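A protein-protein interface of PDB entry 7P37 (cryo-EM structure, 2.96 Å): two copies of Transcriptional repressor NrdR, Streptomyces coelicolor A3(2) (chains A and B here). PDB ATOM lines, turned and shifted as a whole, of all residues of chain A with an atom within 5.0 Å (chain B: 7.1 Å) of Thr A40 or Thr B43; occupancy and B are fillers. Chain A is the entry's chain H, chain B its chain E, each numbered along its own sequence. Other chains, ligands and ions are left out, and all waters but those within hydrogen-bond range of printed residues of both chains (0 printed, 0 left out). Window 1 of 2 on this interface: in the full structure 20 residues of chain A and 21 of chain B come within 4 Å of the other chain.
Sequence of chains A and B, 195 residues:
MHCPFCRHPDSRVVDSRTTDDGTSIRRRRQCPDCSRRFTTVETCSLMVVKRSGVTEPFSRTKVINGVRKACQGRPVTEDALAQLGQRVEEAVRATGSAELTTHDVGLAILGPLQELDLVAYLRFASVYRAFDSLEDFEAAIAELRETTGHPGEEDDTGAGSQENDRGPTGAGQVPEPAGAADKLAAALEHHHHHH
The side-chain carboxylate (OE1) of Glu A42 lies within salt-bridge range of the guanidinium group (NE) of Arg B27 (3.6 Å). The side-chain carboxylate of Glu B42 lies within salt-bridge range of the guanidinium group of Arg A27 (3.3 Å). The side-chain carboxylate (OE2) of Glu B42 lies within salt-bridge range of the guanidinium group (NE) of Arg A29. OE2 of Glu B42 sits at hydrogen-bond distance from OG1 of Thr A40 (2.4 Å). The backbone carbonyl oxygen of Thr B43 lies within hydrogen-bond range of the backbone NH of Val A41. The backbone carbonyl oxygen (O) of Gly B96 lies within hydrogen-bond range of the guanidinium group (NH1) of Arg A26, 3.5 Å away. The backbone carbonyl oxygen of Thr B23 sits close to the side-chain sulfur of Met A1. NH2 of Arg A29 sits close to NH2 of Arg B27, at 3.4 Å.
Met A1 touches Ile B25 (CE to CG1, 3.8 Å). O of Glu B42 touches CE of Met A1, at 3.3 Å. SG of Cys B44 touches SD of Met A1, 3.8 Å away. Arg A29 touches Ile B25 (NH2 to CD1, 3.6 Å). Thr A39 touches Arg B93. Thr B43 touches Thr A40 (O to CB, 3.3 Å). Thr A40 touches Cys B44. Val A41 touches Glu B42. Glu A42 touches Val B41. Glu A42 touches Glu B42.
The backbone carbonyl oxygen (O) of Ile B25 lies within hydrogen-bond range of the backbone NH (N) of Glu B42, 2.9 Å away. The side-chain carboxylate of Glu B42 is in salt-bridge range of the guanidinium group of Arg B27 (3.0 Å). The guanidinium group (NH1) of Arg B93 lies within hydrogen-bond range of the backbone carbonyl oxygen (O) of Cys B44, at 2.7 Å. O of Ile A25 lies within hydrogen-bond range of N of Glu A42, 2.9 Å away. The side-chain carboxylate of Glu A42 lies within salt-bridge range of the guanidinium group of Arg A27, at 2.5 Å. The backbone carbonyl oxygen (O) of Arg A29 sits at hydrogen-bond distance from the backbone NH (N) of Phe A38 (2.9 Å).
Hydrophobic or aromatic side chains of chain B that line the printed part of chain A: Ile B25. Of the 10 printed residues of chain A, 8 touch a printed residue of chain B. Printed residues of chain A that touch a printed residue of chain B: Met A1, Arg A26, Arg A27, Arg A29, Thr A39, Thr A40, Val A41 and Glu A42. Hydrophobic or aromatic side chains of chain A that line the printed part of chain B: Met A1. Among the printed residues, Asp or Glu carboxylates within 4 Å of a Lys or Arg side-chain nitrogen of the other chain: Arg A27 with Glu B42, Arg A29 with Glu B42 and Glu A42 with Arg B27.
Thr A40 touches just these residues of chain B: Glu B42, Thr B43 and Cys B44. Printed residues of chain A within 4 Å of Thr B43: Thr A40 (3.3 Å) and Val A41 (3.2 Å). Printed residues of chain B within 4 Å of Glu A42: Arg B27, Val B41 and Glu B42. Printed residues of chain A within 4 Å of Arg B93: Thr A39. Printed residues of chain B within 4 Å of Thr A39: Cys B44, Arg B93 and Gly B96. Of the printed residues of chain A, Cys B44 touches Met A1, Thr A39 and Thr A40. The nearest residue of chain B that does not touch Thr A40 is Thr B23 (6.2 Å).
Arg A27 touches Glu B42, and with the chains exchanged Glu A42 touches Arg B27. Val B41 touches its own counterpart, Val A41. Val A41 touches Glu B42, and with the chains exchanged Glu A42 touches Val B41. Glu A42 touches its own counterpart, Glu B42.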
ATOM      1  N   MET A   1      26.086  13.029  -5.358  1.00  0.00           N
ATOM      2  CA  MET A   1      25.737  13.964  -6.420  1.00  0.00           C
ATOM      3  C   MET A   1      25.570  15.372  -5.863  1.00  0.00           C
ATOM      4  O   MET A   1      25.002  15.559  -4.790  1.00  0.00           O
ATOM      5  CB  MET A   1      24.456  13.517  -7.127  1.00  0.00           C
ATOM      6  CG  MET A   1      24.062  14.387  -8.306  1.00  0.00           C
ATOM      7  SD  MET A   1      22.583  13.792  -9.142  1.00  0.00           S
ATOM      8  CE  MET A   1      23.208  12.299  -9.900  1.00  0.00           C
ATOM      9  N   ILE A  25      16.100   3.168 -13.011  1.00  0.00           N
ATOM     10  CA  ILE A  25      15.991   3.238 -11.560  1.00  0.00           C
ATOM     11  C   ILE A  25      15.726   4.686 -11.175  1.00  0.00           C
ATOM     12  O   ILE A  25      16.454   5.588 -11.601  1.00  0.00           O
ATOM     13  CB  ILE A  25      17.262   2.717 -10.858  1.00  0.00           C
ATOM     14  CG1 ILE A  25      17.594   1.297 -11.322  1.00  0.00           C
ATOM     15  CG2 ILE A  25      17.090   2.757  -9.350  1.00  0.00           C
ATOM     16  CD1 ILE A  25      18.820   0.712 -10.662  1.00  0.00           C
ATOM     17  N   ARG A  26      14.688   4.912 -10.374  1.00  0.00           N
ATOM     18  CA  ARG A  26      14.308   6.255  -9.953  1.00  0.00           C
ATOM     19  C   ARG A  26      14.597   6.400  -8.467  1.00  0.00           C
ATOM     20  O   ARG A  26      14.085   5.626  -7.654  1.00  0.00           O
ATOM     21  CB  ARG A  26      12.833   6.527 -10.252  1.00  0.00           C
ATOM     22  CG  ARG A  26      12.511   6.544 -11.736  1.00  0.00           C
ATOM     23  CD  ARG A  26      11.147   7.149 -12.009  1.00  0.00           C
ATOM     24  NE  ARG A  26      10.969   7.453 -13.424  1.00  0.00           N
ATOM     25  CZ  ARG A  26      11.272   8.616 -13.984  1.00  0.00           C
ATOM     26  NH1 ARG A  26      11.764   9.617 -13.274  1.00  0.00           N
ATOM     27  NH2 ARG A  26      11.079   8.779 -15.290  1.00  0.00           N
ATOM     28  N   ARG A  27      15.414   7.390  -8.117  1.00  0.00           N
ATOM     29  CA  ARG A  27      15.808   7.623  -6.739  1.00  0.00           C
ATOM     30  C   ARG A  27      15.370   9.009  -6.294  1.00  0.00           C
ATOM     31  O   ARG A  27      15.374   9.964  -7.077  1.00  0.00           O
ATOM     32  CB  ARG A  27      17.325   7.487  -6.556  1.00  0.00           C
ATOM     33  CG  ARG A  27      17.884   6.107  -6.850  1.00  0.00           C
ATOM     34  CD  ARG A  27      19.385   6.074  -6.619  1.00  0.00           C
ATOM     35  NE  ARG A  27      19.959   4.759  -6.872  1.00  0.00           N
ATOM     36  CZ  ARG A  27      20.468   4.374  -8.033  1.00  0.00           C
ATOM     37  NH1 ARG A  27      20.487   5.182  -9.081  1.00  0.00           N
ATOM     38  NH2 ARG A  27      20.973   3.150  -8.146  1.00  0.00           N
ATOM     39  N   ARG A  29      16.493  11.812  -3.526  1.00  0.00           N
ATOM     40  CA  ARG A  29      17.676  12.202  -2.779  1.00  0.00           C
ATOM     41  C   ARG A  29      17.389  13.466  -1.981  1.00  0.00           C
ATOM     42  O   ARG A  29      16.498  14.248  -2.320  1.00  0.00           O
ATOM     43  CB  ARG A  29      18.864  12.448  -3.717  1.00  0.00           C
ATOM     44  CG  ARG A  29      19.259  11.251  -4.556  1.00  0.00           C
ATOM     45  CD  ARG A  29      20.416  11.593  -5.475  1.00  0.00           C
ATOM     46  NE  ARG A  29      21.049  10.400  -6.026  1.00  0.00           N
ATOM     47  CZ  ARG A  29      22.139   9.835  -5.527  1.00  0.00           C
ATOM     48  NH1 ARG A  29      22.754  10.333  -4.467  1.00  0.00           N
ATOM     49  NH2 ARG A  29      22.627   8.742  -6.107  1.00  0.00           N
ATOM     50  N   PHE A  38      15.266  16.167  -4.110  1.00  0.00           N
ATOM     51  CA  PHE A  38      15.111  16.149  -5.558  1.00  0.00           C
ATOM     52  C   PHE A  38      15.096  14.697  -6.021  1.00  0.00           C
ATOM     53  O   PHE A  38      15.171  13.767  -5.212  1.00  0.00           O
ATOM     54  CB  PHE A  38      16.204  16.974  -6.254  1.00  0.00           C
ATOM     55  CG  PHE A  38      17.608  16.509  -5.969  1.00  0.00           C
ATOM     56  CD1 PHE A  38      18.191  16.719  -4.730  1.00  0.00           C
ATOM     57  CD2 PHE A  38      18.354  15.885  -6.953  1.00  0.00           C
ATOM     58  CE1 PHE A  38      19.482  16.300  -4.475  1.00  0.00           C
ATOM     59  CE2 PHE A  38      19.646  15.465  -6.704  1.00  0.00           C
ATOM     60  CZ  PHE A  38      20.209  15.672  -5.464  1.00  0.00           C
ATOM     61  N   THR A  39      14.980  14.503  -7.333  1.00  0.00           N
ATOM     62  CA  THR A  39      14.842  13.171  -7.904  1.00  0.00           C
ATOM     63  C   THR A  39      15.854  12.969  -9.025  1.00  0.00           C
ATOM     64  O   THR A  39      16.243  13.916  -9.715  1.00  0.00           O
ATOM     65  CB  THR A  39      13.420  12.932  -8.436  1.00  0.00           C
ATOM     66  OG1 THR A  39      13.305  11.586  -8.916  1.00  0.00           O
ATOM     67  CG2 THR A  39      13.098  13.892  -9.565  1.00  0.00           C
ATOM     68  N   THR A  40      16.288  11.719  -9.184  1.00  0.00           N
ATOM     69  CA  THR A  40      17.236  11.340 -10.219  1.00  0.00           C
ATOM     70  C   THR A  40      16.774  10.049 -10.880  1.00  0.00           C
ATOM     71  O   THR A  40      16.075   9.237 -10.269  1.00  0.00           O
ATOM     72  CB  THR A  40      18.653  11.145  -9.661  1.00  0.00           C
ATOM     73  OG1 THR A  40      18.628  10.159  -8.622  1.00  0.00           O
ATOM     74  CG2 THR A  40      19.199  12.448  -9.105  1.00  0.00           C
ATOM     75  N   VAL A  41      17.178   9.866 -12.135  1.00  0.00           N
ATOM     76  CA  VAL A  41      16.874   8.660 -12.896  1.00  0.00           C
ATOM     77  C   VAL A  41      18.173   8.119 -13.484  1.00  0.00           C
ATOM     78  O   VAL A  41      18.983   8.878 -14.026  1.00  0.00           O
ATOM     79  CB  VAL A  41      15.827   8.922 -13.999  1.00  0.00           C
ATOM     80  CG1 VAL A  41      16.315   9.969 -14.990  1.00  0.00           C
ATOM     81  CG2 VAL A  41      15.472   7.628 -14.714  1.00  0.00           C
ATOM     82  N   GLU A  42      18.382   6.812 -13.344  1.00  0.00           N
ATOM     83  CA  GLU A  42      19.562   6.131 -13.856  1.00  0.00           C
ATOM     84  C   GLU A  42      19.124   5.109 -14.896  1.00  0.00           C
ATOM     85  O   GLU A  42      18.289   4.246 -14.608  1.00  0.00           O
ATOM     86  CB  GLU A  42      20.334   5.447 -12.730  1.00  0.00           C
ATOM     87  CG  GLU A  42      21.385   4.463 -13.207  1.00  0.00           C
ATOM     88  CD  GLU A  42      22.000   3.672 -12.072  1.00  0.00           C
ATOM     89  OE1 GLU A  42      21.662   3.950 -10.902  1.00  0.00           O
ATOM     90  OE2 GLU A  42      22.823   2.774 -12.350  1.00  0.00           O
ATOM     91  N   THR B  23      27.061  16.790 -11.769  1.00  0.00           N
ATOM     92  CA  THR B  23      25.691  16.641 -12.241  1.00  0.00           C
ATOM     93  C   THR B  23      25.258  15.179 -12.280  1.00  0.00           C
ATOM     94  O   THR B  23      24.119  14.857 -11.928  1.00  0.00           O
ATOM     95  CB  THR B  23      25.543  17.272 -13.625  1.00  0.00           C
ATOM     96  OG1 THR B  23      26.070  18.605 -13.602  1.00  0.00           O
ATOM     97  CG2 THR B  23      24.079  17.321 -14.036  1.00  0.00           C
ATOM     98  N   SER B  24      26.152  14.282 -12.689  1.00  0.00           N
ATOM     99  CA  SER B  24      25.809  12.889 -12.923  1.00  0.00           C
ATOM    100  C   SER B  24      26.753  11.974 -12.155  1.00  0.00           C
ATOM    101  O   SER B  24      27.848  12.369 -11.754  1.00  0.00           O
ATOM    102  CB  SER B  24      25.861  12.548 -14.417  1.00  0.00           C
ATOM    103  OG  SER B  24      27.162  12.746 -14.939  1.00  0.00           O
ATOM    104  N   ILE B  25      26.300  10.740 -11.949  1.00  0.00           N
ATOM    105  CA  ILE B  25      27.105   9.683 -11.345  1.00  0.00           C
ATOM    106  C   ILE B  25      27.201   8.546 -12.351  1.00  0.00           C
ATOM    107  O   ILE B  25      26.176   8.039 -12.819  1.00  0.00           O
ATOM    108  CB  ILE B  25      26.504   9.187 -10.021  1.00  0.00           C
ATOM    109  CG1 ILE B  25      26.299  10.350  -9.052  1.00  0.00           C
ATOM    110  CG2 ILE B  25      27.391   8.123  -9.401  1.00  0.00           C
ATOM    111  CD1 ILE B  25      25.655   9.943  -7.748  1.00  0.00           C
ATOM    112  N   ARG B  27      28.160   4.743 -13.057  1.00  0.00           N
ATOM    113  CA  ARG B  27      28.330   3.464 -12.390  1.00  0.00           C
ATOM    114  C   ARG B  27      28.644   2.384 -13.414  1.00  0.00           C
ATOM    115  O   ARG B  27      28.208   2.450 -14.566  1.00  0.00           O
ATOM    116  CB  ARG B  27      27.077   3.072 -11.598  1.00  0.00           C
ATOM    117  CG  ARG B  27      26.707   4.037 -10.488  1.00  0.00           C
ATOM    118  CD  ARG B  27      25.333   3.715  -9.932  1.00  0.00           C
ATOM    119  NE  ARG B  27      24.753   4.840  -9.210  1.00  0.00           N
ATOM    120  CZ  ARG B  27      24.655   4.911  -7.891  1.00  0.00           C
ATOM    121  NH1 ARG B  27      25.087   3.934  -7.112  1.00  0.00           N
ATOM    122  NH2 ARG B  27      24.106   5.988  -7.337  1.00  0.00           N
ATOM    123  N   VAL B  41      24.450   5.793 -16.265  1.00  0.00           N
ATOM    124  CA  VAL B  41      24.631   7.181 -15.857  1.00  0.00           C
ATOM    125  C   VAL B  41      23.368   7.645 -15.146  1.00  0.00           C
ATOM    126  O   VAL B  41      22.257   7.428 -15.641  1.00  0.00           O
ATOM    127  CB  VAL B  41      24.944   8.095 -17.057  1.00  0.00           C
ATOM    128  CG1 VAL B  41      25.099   9.535 -16.601  1.00  0.00           C
ATOM    129  CG2 VAL B  41      26.199   7.623 -17.767  1.00  0.00           C
ATOM    130  N   GLU B  42      23.541   8.279 -13.989  1.00  0.00           N
ATOM    131  CA  GLU B  42      22.444   8.837 -13.211  1.00  0.00           C
ATOM    132  C   GLU B  42      22.524  10.355 -13.254  1.00  0.00           C
ATOM    133  O   GLU B  42      23.568  10.933 -12.933  1.00  0.00           O
ATOM    134  CB  GLU B  42      22.495   8.345 -11.764  1.00  0.00           C
ATOM    135  CG  GLU B  42      21.557   9.075 -10.829  1.00  0.00           C
ATOM    136  CD  GLU B  42      21.587   8.513  -9.424  1.00  0.00           C
ATOM    137  OE1 GLU B  42      22.555   7.801  -9.088  1.00  0.00           O
ATOM    138  OE2 GLU B  42      20.642   8.781  -8.654  1.00  0.00           O
ATOM    139  N   THR B  43      21.425  10.996 -13.644  1.00  0.00           N
ATOM    140  CA  THR B  43      21.379  12.437 -13.836  1.00  0.00           C
ATOM    141  C   THR B  43      20.169  13.018 -13.113  1.00  0.00           C
ATOM    142  O   THR B  43      19.235  12.306 -12.739  1.00  0.00           O
ATOM    143  CB  THR B  43      21.318  12.808 -15.323  1.00  0.00           C
ATOM    144  OG1 THR B  43      20.219  12.129 -15.941  1.00  0.00           O
ATOM    145  CG2 THR B  43      22.607  12.421 -16.026  1.00  0.00           C
ATOM    146  N   CYS B  44      20.203  14.334 -12.922  1.00  0.00           N
ATOM    147  CA  CYS B  44      19.104  15.099 -12.347  1.00  0.00           C
ATOM    148  C   CYS B  44      18.757  16.278 -13.243  1.00  0.00           C
ATOM    149  O   CYS B  44      18.315  17.332 -12.776  1.00  0.00           O
ATOM    150  CB  CYS B  44      19.444  15.575 -10.937  1.00  0.00           C
ATOM    151  SG  CYS B  44      20.822  16.741 -10.845  1.00  0.00           S
ATOM    152  N   SER B  45      18.957  16.114 -14.548  1.00  0.00           N
ATOM    153  CA  SER B  45      18.734  17.201 -15.491  1.00  0.00           C
ATOM    154  C   SER B  45      17.252  17.541 -15.595  1.00  0.00           C
ATOM    155  O   SER B  45      16.381  16.671 -15.515  1.00  0.00           O
ATOM    156  CB  SER B  45      19.285  16.832 -16.866  1.00  0.00           C
ATOM    157  OG  SER B  45      19.165  17.917 -17.769  1.00  0.00           O
ATOM    158  N   ARG B  93      10.851  20.006  -9.499  1.00  0.00           N
ATOM    159  CA  ARG B  93      11.629  18.773  -9.520  1.00  0.00           C
ATOM    160  C   ARG B  93      10.912  17.625  -8.820  1.00  0.00           C
ATOM    161  O   ARG B  93      11.197  16.459  -9.113  1.00  0.00           O
ATOM    162  CB  ARG B  93      12.998  19.000  -8.879  1.00  0.00           C
ATOM    163  CG  ARG B  93      13.903  19.929  -9.665  1.00  0.00           C
ATOM    164  CD  ARG B  93      15.299  19.976  -9.069  1.00  0.00           C
ATOM    165  NE  ARG B  93      16.218  20.752  -9.893  1.00  0.00           N
ATOM    166  CZ  ARG B  93      16.955  20.246 -10.870  1.00  0.00           C
ATOM    167  NH1 ARG B  93      16.909  18.959 -11.176  1.00  0.00           N
ATOM    168  NH2 ARG B  93      17.761  21.049 -11.558  1.00  0.00           N
ATOM    169  N   GLY B  96       9.175  14.730 -10.940  1.00  0.00           N
ATOM    170  CA  GLY B  96       9.971  13.674 -11.525  1.00  0.00           C
ATOM    171  C   GLY B  96      10.105  13.729 -13.031  1.00  0.00           C
ATOM    172  O   GLY B  96      10.876  12.942 -13.595  1.00  0.00           O
